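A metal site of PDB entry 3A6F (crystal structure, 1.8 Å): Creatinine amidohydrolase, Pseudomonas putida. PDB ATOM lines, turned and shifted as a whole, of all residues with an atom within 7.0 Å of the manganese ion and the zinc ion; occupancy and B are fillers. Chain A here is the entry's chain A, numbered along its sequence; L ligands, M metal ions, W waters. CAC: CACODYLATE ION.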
ATOM      1  N   GLY A  31     -21.150  24.796  17.889  1.00  0.00           N
ATOM      2  CA  GLY A  31     -19.898  24.145  18.228  1.00  0.00           C
ATOM      3  C   GLY A  31     -18.751  24.307  17.248  1.00  0.00           C
ATOM      4  O   GLY A  31     -18.494  25.394  16.732  1.00  0.00           O
ATOM      5  N   ALA A  32     -18.060  23.192  17.000  1.00  0.00           N
ATOM      6  CA  ALA A  32     -16.927  23.182  16.097  1.00  0.00           C
ATOM      7  C   ALA A  32     -16.394  21.767  15.930  1.00  0.00           C
ATOM      8  O   ALA A  32     -16.752  20.869  16.695  1.00  0.00           O
ATOM      9  CB  ALA A  32     -15.807  24.070  16.668  1.00  0.00           C
ATOM     10  N   GLU A  34     -12.943  20.358  16.057  1.00  0.00           N
ATOM     11  CA  GLU A  34     -11.606  20.794  16.454  1.00  0.00           C
ATOM     12  C   GLU A  34     -10.868  19.692  17.223  1.00  0.00           C
ATOM     13  O   GLU A  34     -11.482  18.924  17.957  1.00  0.00           O
ATOM     14  CB  GLU A  34     -11.764  22.038  17.328  1.00  0.00           C
ATOM     15  CG  GLU A  34     -10.505  22.650  17.909  1.00  0.00           C
ATOM     16  CD  GLU A  34     -10.840  23.771  18.864  1.00  0.00           C
ATOM     17  OE1 GLU A  34     -11.741  23.572  19.704  1.00  0.00           O
ATOM     18  OE2 GLU A  34     -10.218  24.850  18.800  1.00  0.00           O
ATOM     19  N   GLN A  35      -9.548  19.612  17.039  1.00  0.00           N
ATOM     20  CA  GLN A  35      -8.770  18.597  17.725  1.00  0.00           C
ATOM     21  C   GLN A  35      -8.907  18.791  19.226  1.00  0.00           C
ATOM     22  O   GLN A  35      -9.053  19.922  19.691  1.00  0.00           O
ATOM     23  CB  GLN A  35      -7.290  18.667  17.320  1.00  0.00           C
ATOM     24  CG  GLN A  35      -6.526  19.935  17.721  1.00  0.00           C
ATOM     25  CD  GLN A  35      -6.163  19.989  19.195  1.00  0.00           C
ATOM     26  OE1 GLN A  35      -5.886  18.971  19.834  1.00  0.00           O
ATOM     27  NE2 GLN A  35      -6.146  21.202  19.759  1.00  0.00           N
ATOM     28  N   HIS A  36      -8.882  17.699  19.974  1.00  0.00           N
ATOM     29  CA  HIS A  36      -8.984  17.723  21.427  1.00  0.00           C
ATOM     30  C   HIS A  36      -8.021  16.738  22.094  1.00  0.00           C
ATOM     31  O   HIS A  36      -8.428  15.947  22.955  1.00  0.00           O
ATOM     32  CB  HIS A  36     -10.414  17.428  21.885  1.00  0.00           C
ATOM     33  CG  HIS A  36     -11.295  18.630  21.917  1.00  0.00           C
ATOM     34  ND1 HIS A  36     -11.712  19.277  20.773  1.00  0.00           N
ATOM     35  CD2 HIS A  36     -11.787  19.343  22.963  1.00  0.00           C
ATOM     36  CE1 HIS A  36     -12.421  20.349  21.117  1.00  0.00           C
ATOM     37  NE2 HIS A  36     -12.470  20.407  22.427  1.00  0.00           N
ATOM     38  N   MET A  40      -9.445  12.443  23.237  1.00  0.00           N
ATOM     39  CA  MET A  40     -10.854  12.692  22.902  1.00  0.00           C
ATOM     40  C   MET A  40     -11.135  12.919  21.425  1.00  0.00           C
ATOM     41  O   MET A  40     -10.235  13.242  20.645  1.00  0.00           O
ATOM     42  CB  MET A  40     -11.383  13.910  23.678  1.00  0.00           C
ATOM     43  CG  MET A  40     -11.511  13.706  25.168  1.00  0.00           C
ATOM     44  SD  MET A  40     -12.639  14.915  25.887  1.00  0.00           S
ATOM     45  CE  MET A  40     -11.640  16.412  25.785  1.00  0.00           C
ATOM     46  N   VAL A  44     -16.323  17.342  20.211  1.00  0.00           N
ATOM     47  CA  VAL A  44     -16.639  17.698  21.595  1.00  0.00           C
ATOM     48  C   VAL A  44     -17.448  19.005  21.710  1.00  0.00           C
ATOM     49  O   VAL A  44     -18.463  19.051  22.414  1.00  0.00           O
ATOM     50  CB  VAL A  44     -15.343  17.825  22.452  1.00  0.00           C
ATOM     51  CG1 VAL A  44     -15.672  18.366  23.846  1.00  0.00           C
ATOM     52  CG2 VAL A  44     -14.659  16.461  22.566  1.00  0.00           C
ATOM     53  N   ASP A  45     -17.016  20.052  21.024  1.00  0.00           N
ATOM     54  CA  ASP A  45     -17.710  21.340  21.104  1.00  0.00           C
ATOM     55  C   ASP A  45     -19.138  21.364  20.587  1.00  0.00           C
ATOM     56  O   ASP A  45     -19.844  22.362  20.762  1.00  0.00           O
ATOM     57  CB  ASP A  45     -16.886  22.423  20.424  1.00  0.00           C
ATOM     58  CG  ASP A  45     -15.583  22.655  21.138  1.00  0.00           C
ATOM     59  OD1 ASP A  45     -15.467  22.193  22.289  1.00  0.00           O
ATOM     60  OD2 ASP A  45     -14.684  23.284  20.563  1.00  0.00           O
ATOM     61  N   LEU A  48     -21.116  18.613  23.690  1.00  0.00           N
ATOM     62  CA  LEU A  48     -21.377  19.177  25.010  1.00  0.00           C
ATOM     63  C   LEU A  48     -22.496  20.217  25.095  1.00  0.00           C
ATOM     64  O   LEU A  48     -23.424  20.063  25.889  1.00  0.00           O
ATOM     65  CB  LEU A  48     -20.071  19.738  25.608  1.00  0.00           C
ATOM     66  CG  LEU A  48     -18.962  18.699  25.842  1.00  0.00           C
ATOM     67  CD1 LEU A  48     -17.816  19.315  26.629  1.00  0.00           C
ATOM     68  CD2 LEU A  48     -19.518  17.501  26.595  1.00  0.00           C
ATOM     69  N   TYR A  72     -15.613  28.954  14.209  1.00  0.00           N
ATOM     70  CA  TYR A  72     -14.521  29.820  13.788  1.00  0.00           C
ATOM     71  C   TYR A  72     -13.148  29.206  14.037  1.00  0.00           C
ATOM     72  O   TYR A  72     -12.986  28.314  14.864  1.00  0.00           O
ATOM     73  CB  TYR A  72     -14.616  31.183  14.479  1.00  0.00           C
ATOM     74  CG  TYR A  72     -13.561  32.124  13.967  1.00  0.00           C
ATOM     75  CD1 TYR A  72     -13.545  32.519  12.623  1.00  0.00           C
ATOM     76  CD2 TYR A  72     -12.523  32.553  14.786  1.00  0.00           C
ATOM     77  CE1 TYR A  72     -12.535  33.316  12.120  1.00  0.00           C
ATOM     78  CE2 TYR A  72     -11.503  33.355  14.302  1.00  0.00           C
ATOM     79  CZ  TYR A  72     -11.518  33.730  12.954  1.00  0.00           C
ATOM     80  OH  TYR A  72     -10.512  34.518  12.450  1.00  0.00           O
ATOM     81  N   SER A  74      -9.671  27.964  15.091  1.00  0.00           N
ATOM     82  CA  SER A  74      -9.102  27.665  16.394  1.00  0.00           C
ATOM     83  C   SER A  74      -7.924  28.597  16.671  1.00  0.00           C
ATOM     84  O   SER A  74      -7.058  28.789  15.810  1.00  0.00           O
ATOM     85  CB  SER A  74      -8.629  26.205  16.413  1.00  0.00           C
ATOM     86  OG  SER A  74      -8.106  25.851  17.678  1.00  0.00           O
ATOM     87  N   SER A  78      -6.470  29.348  22.940  1.00  0.00           N
ATOM     88  CA  SER A  78      -7.735  28.808  23.417  1.00  0.00           C
ATOM     89  C   SER A  78      -8.038  27.397  22.926  1.00  0.00           C
ATOM     90  O   SER A  78      -8.569  26.585  23.675  1.00  0.00           O
ATOM     91  CB  SER A  78      -8.884  29.754  23.059  1.00  0.00           C
ATOM     92  OG  SER A  78      -8.882  30.081  21.684  1.00  0.00           O
ATOM     93  N   GLY A  79      -7.697  27.108  21.678  1.00  0.00           N
ATOM     94  CA  GLY A  79      -7.969  25.795  21.131  1.00  0.00           C
ATOM     95  C   GLY A  79      -6.745  25.096  20.549  1.00  0.00           C
ATOM     96  O   GLY A  79      -6.873  24.047  19.919  1.00  0.00           O
ATOM     97  N   GLY A 119     -20.347  26.440  22.336  1.00  0.00           N
ATOM     98  CA  GLY A 119     -19.554  25.365  22.895  1.00  0.00           C
ATOM     99  C   GLY A 119     -18.093  25.485  22.486  1.00  0.00           C
ATOM    100  O   GLY A 119     -17.241  24.707  22.923  1.00  0.00           O
ATOM    101  N   HIS A 120     -17.808  26.490  21.650  1.00  0.00           N
ATOM    102  CA  HIS A 120     -16.471  26.751  21.110  1.00  0.00           C
ATOM    103  C   HIS A 120     -16.079  28.222  21.364  1.00  0.00           C
ATOM    104  O   HIS A 120     -16.591  29.135  20.712  1.00  0.00           O
ATOM    105  CB  HIS A 120     -16.500  26.425  19.619  1.00  0.00           C
ATOM    106  CG  HIS A 120     -15.208  26.653  18.893  1.00  0.00           C
ATOM    107  ND1 HIS A 120     -14.018  26.064  19.279  1.00  0.00           N
ATOM    108  CD2 HIS A 120     -14.934  27.342  17.756  1.00  0.00           C
ATOM    109  CE1 HIS A 120     -13.074  26.368  18.403  1.00  0.00           C
ATOM    110  NE2 HIS A 120     -13.605  27.149  17.470  1.00  0.00           N
ATOM    111  N   TYR A 121     -15.183  28.427  22.318  1.00  0.00           N
ATOM    112  CA  TYR A 121     -14.734  29.772  22.698  1.00  0.00           C
ATOM    113  C   TYR A 121     -14.611  30.785  21.564  1.00  0.00           C
ATOM    114  O   TYR A 121     -15.157  31.880  21.636  1.00  0.00           O
ATOM    115  CB  TYR A 121     -13.388  29.677  23.424  1.00  0.00           C
ATOM    116  CG  TYR A 121     -12.947  30.984  24.049  1.00  0.00           C
ATOM    117  CD1 TYR A 121     -13.586  31.477  25.189  1.00  0.00           C
ATOM    118  CD2 TYR A 121     -11.913  31.722  23.492  1.00  0.00           C
ATOM    119  CE1 TYR A 121     -13.188  32.687  25.765  1.00  0.00           C
ATOM    120  CE2 TYR A 121     -11.506  32.929  24.065  1.00  0.00           C
ATOM    121  CZ  TYR A 121     -12.152  33.403  25.203  1.00  0.00           C
ATOM    122  OH  TYR A 121     -11.752  34.603  25.765  1.00  0.00           O
ATOM    123  N   GLU A 122     -13.878  30.421  20.515  1.00  0.00           N
ATOM    124  CA  GLU A 122     -13.671  31.297  19.366  1.00  0.00           C
ATOM    125  C   GLU A 122     -14.909  31.761  18.602  1.00  0.00           C
ATOM    126  O   GLU A 122     -14.827  32.709  17.817  1.00  0.00           O
ATOM    127  CB  GLU A 122     -12.684  30.641  18.391  1.00  0.00           C
ATOM    128  CG  GLU A 122     -11.264  30.466  18.955  1.00  0.00           C
ATOM    129  CD  GLU A 122     -11.077  29.181  19.755  1.00  0.00           C
ATOM    130  OE1 GLU A 122     -12.050  28.725  20.393  1.00  0.00           O
ATOM    131  OE2 GLU A 122      -9.952  28.646  19.764  1.00  0.00           O
ATOM    132  N   ASN A 123     -16.047  31.109  18.803  1.00  0.00           N
ATOM    133  CA  ASN A 123     -17.268  31.488  18.091  1.00  0.00           C
ATOM    134  C   ASN A 123     -17.930  32.781  18.529  1.00  0.00           C
ATOM    135  O   ASN A 123     -18.525  33.480  17.721  1.00  0.00           O
ATOM    136  CB  ASN A 123     -18.330  30.387  18.213  1.00  0.00           C
ATOM    137  CG  ASN A 123     -17.954  29.115  17.494  1.00  0.00           C
ATOM    138  OD1 ASN A 123     -17.275  29.144  16.460  1.00  0.00           O
ATOM    139  ND2 ASN A 123     -18.431  27.991  18.006  1.00  0.00           N
ATOM    140  N   TYR A 153     -21.996  27.664  27.958  1.00  0.00           N
ATOM    141  CA  TYR A 153     -22.349  26.873  29.124  1.00  0.00           C
ATOM    142  C   TYR A 153     -21.341  26.871  30.286  1.00  0.00           C
ATOM    143  O   TYR A 153     -21.742  26.921  31.452  1.00  0.00           O
ATOM    144  CB  TYR A 153     -22.686  25.437  28.705  1.00  0.00           C
ATOM    145  CG  TYR A 153     -21.510  24.605  28.275  1.00  0.00           C
ATOM    146  CD1 TYR A 153     -20.788  23.849  29.209  1.00  0.00           C
ATOM    147  CD2 TYR A 153     -21.096  24.573  26.946  1.00  0.00           C
ATOM    148  CE1 TYR A 153     -19.688  23.095  28.834  1.00  0.00           C
ATOM    149  CE2 TYR A 153     -19.978  23.824  26.554  1.00  0.00           C
ATOM    150  CZ  TYR A 153     -19.287  23.089  27.504  1.00  0.00           C
ATOM    151  OH  TYR A 153     -18.182  22.364  27.144  1.00  0.00           O
ATOM    152  N   TRP A 154     -20.049  26.831  29.981  1.00  0.00           N
ATOM    153  CA  TRP A 154     -19.043  26.805  31.052  1.00  0.00           C
ATOM    154  C   TRP A 154     -19.049  28.008  31.991  1.00  0.00           C
ATOM    155  O   TRP A 154     -18.599  27.905  33.129  1.00  0.00           O
ATOM    156  CB  TRP A 154     -17.635  26.605  30.454  1.00  0.00           C
ATOM    157  CG  TRP A 154     -17.175  27.691  29.539  1.00  0.00           C
ATOM    158  CD1 TRP A 154     -16.700  28.921  29.885  1.00  0.00           C
ATOM    159  CD2 TRP A 154     -17.144  27.637  28.105  1.00  0.00           C
ATOM    160  NE1 TRP A 154     -16.375  29.644  28.758  1.00  0.00           N
ATOM    161  CE2 TRP A 154     -16.647  28.877  27.654  1.00  0.00           C
ATOM    162  CE3 TRP A 154     -17.505  26.666  27.164  1.00  0.00           C
ATOM    163  CZ2 TRP A 154     -16.482  29.165  26.288  1.00  0.00           C
ATOM    164  CZ3 TRP A 154     -17.349  26.957  25.802  1.00  0.00           C
ATOM    165  CH2 TRP A 154     -16.835  28.199  25.388  1.00  0.00           C
ATOM    166  N   GLU A 177      -8.315  25.475  29.761  1.00  0.00           N
ATOM    167  CA  GLU A 177      -9.256  24.375  29.687  1.00  0.00           C
ATOM    168  C   GLU A 177      -9.676  23.932  28.282  1.00  0.00           C
ATOM    169  O   GLU A 177     -10.847  24.053  27.910  1.00  0.00           O
ATOM    170  CB  GLU A 177     -10.515  24.684  30.515  1.00  0.00           C
ATOM    171  CG  GLU A 177     -10.351  24.509  32.024  1.00  0.00           C
ATOM    172  CD  GLU A 177      -9.967  23.095  32.432  1.00  0.00           C
ATOM    173  OE1 GLU A 177     -10.449  22.134  31.809  1.00  0.00           O
ATOM    174  OE2 GLU A 177      -9.198  22.940  33.400  1.00  0.00           O
ATOM    175  N   HIS A 178      -8.718  23.454  27.496  1.00  0.00           N
ATOM    176  CA  HIS A 178      -9.022  22.939  26.175  1.00  0.00           C
ATOM    177  C   HIS A 178      -8.604  21.480  26.171  1.00  0.00           C
ATOM    178  O   HIS A 178      -7.409  21.180  26.106  1.00  0.00           O
ATOM    179  CB  HIS A 178      -8.269  23.684  25.070  1.00  0.00           C
ATOM    180  CG  HIS A 178      -8.444  23.061  23.711  1.00  0.00           C
ATOM    181  ND1 HIS A 178      -9.670  22.963  23.096  1.00  0.00           N
ATOM    182  CD2 HIS A 178      -7.560  22.442  22.890  1.00  0.00           C
ATOM    183  CE1 HIS A 178      -9.539  22.317  21.957  1.00  0.00           C
ATOM    184  NE2 HIS A 178      -8.277  21.988  21.808  1.00  0.00           N
ATOM    185  N   GLY A 179      -9.575  20.584  26.238  1.00  0.00           N
ATOM    186  CA  GLY A 179      -9.265  19.162  26.270  1.00  0.00           C
ATOM    187  C   GLY A 179      -8.714  18.790  27.640  1.00  0.00           C
ATOM    188  O   GLY A 179      -8.092  17.744  27.811  1.00  0.00           O
ATOM    189  N   GLU A 183     -13.650  19.671  30.177  1.00  0.00           N
ATOM    190  CA  GLU A 183     -14.322  19.021  29.059  1.00  0.00           C
ATOM    191  C   GLU A 183     -14.236  17.498  29.129  1.00  0.00           C
ATOM    192  O   GLU A 183     -15.200  16.799  28.823  1.00  0.00           O
ATOM    193  CB  GLU A 183     -13.737  19.493  27.730  1.00  0.00           C
ATOM    194  CG  GLU A 183     -14.211  20.856  27.311  1.00  0.00           C
ATOM    195  CD  GLU A 183     -13.756  21.198  25.915  1.00  0.00           C
ATOM    196  OE1 GLU A 183     -14.564  21.778  25.182  1.00  0.00           O
ATOM    197  OE2 GLU A 183     -12.591  20.899  25.569  1.00  0.00           O
HETATM  198 AS   CAC L   1     -13.158  25.254  23.927  1.00  0.00          AS
HETATM  199  O1  CAC L   1     -12.431  23.839  23.234  1.00  0.00           O
HETATM  200  O2  CAC L   1     -13.985  26.096  22.659  1.00  0.00           O
HETATM  201  C1  CAC L   1     -14.499  24.805  25.286  1.00  0.00           C
HETATM  202  C2  CAC L   1     -11.776  26.476  24.603  1.00  0.00           C
HETATM  203 MN    MN M   1     -13.134  24.803  20.872  1.00  0.00          MN
HETATM  204 ZN    ZN M   2     -13.553  21.961  23.323  1.00  0.00          ZN
HETATM  205  O   HOH W   1     -11.247  26.125  21.266  1.00  0.00           O
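NE2 of His 120 lies within hydrogen-bond range of O of Tyr 72, at 2.9 Å.
A ring nitrogen (ND1) of His 120 sits close to the side-chain carboxylate (OE1) of Glu 122, 3.5 Å away.
OE2 of Glu 183 is in hydrogen-bond range of N of Gly 179 (3.1 Å).
The side-chain carboxylate (OE2) of Glu 34 sits at hydrogen-bond distance from the side-chain hydroxyl (OG) of Ser 74 (2.6 Å).
O of His 120 sits close to ND2 of Asn 123 (3.5 Å).
ND1 of His 36 sits at hydrogen-bond distance from O of Glu 34, at 2.8 Å.
Of the 24 residues printed, 3 come within 4 Å of the manganese ion.
Along chain A the residues within 4 Å of the manganese ion span positions 34 to 120.
Three residues have an atom within 4 Å of the zinc ion: His 36, Asp 45 and Glu 183.
OD2 of Asp 45 binds the manganese ion (2.2 Å).
OE1 of Glu 34 binds the manganese ion, 2.2 Å away.
The manganese ion is bound by ND1 of His 120, at 2.2 Å.
Water W1 binds the manganese ion (2.3 Å).
O2 of the ligand is bound to the manganese ion.
The manganese ion is bound by an oxygen (O1) of the ligand (2.6 Å).
The zinc ion is bound by a ring nitrogen (NE2) of His 36, the side-chain carboxylate of Glu 183, the side-chain carboxylate of Asp 45 and an oxygen (O1) of the ligand.
The zinc ion has four donor atoms within binding distance.
Slightly farther from the zinc ion lies OE2 of Glu 183 (2.7 Å).
Water W1 lies within hydrogen-bond range of the side-chain carboxylate (OE1) of Glu 122 (2.9 Å) and the side-chain carboxylate (OE2) of Glu 34 (3.0 Å).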
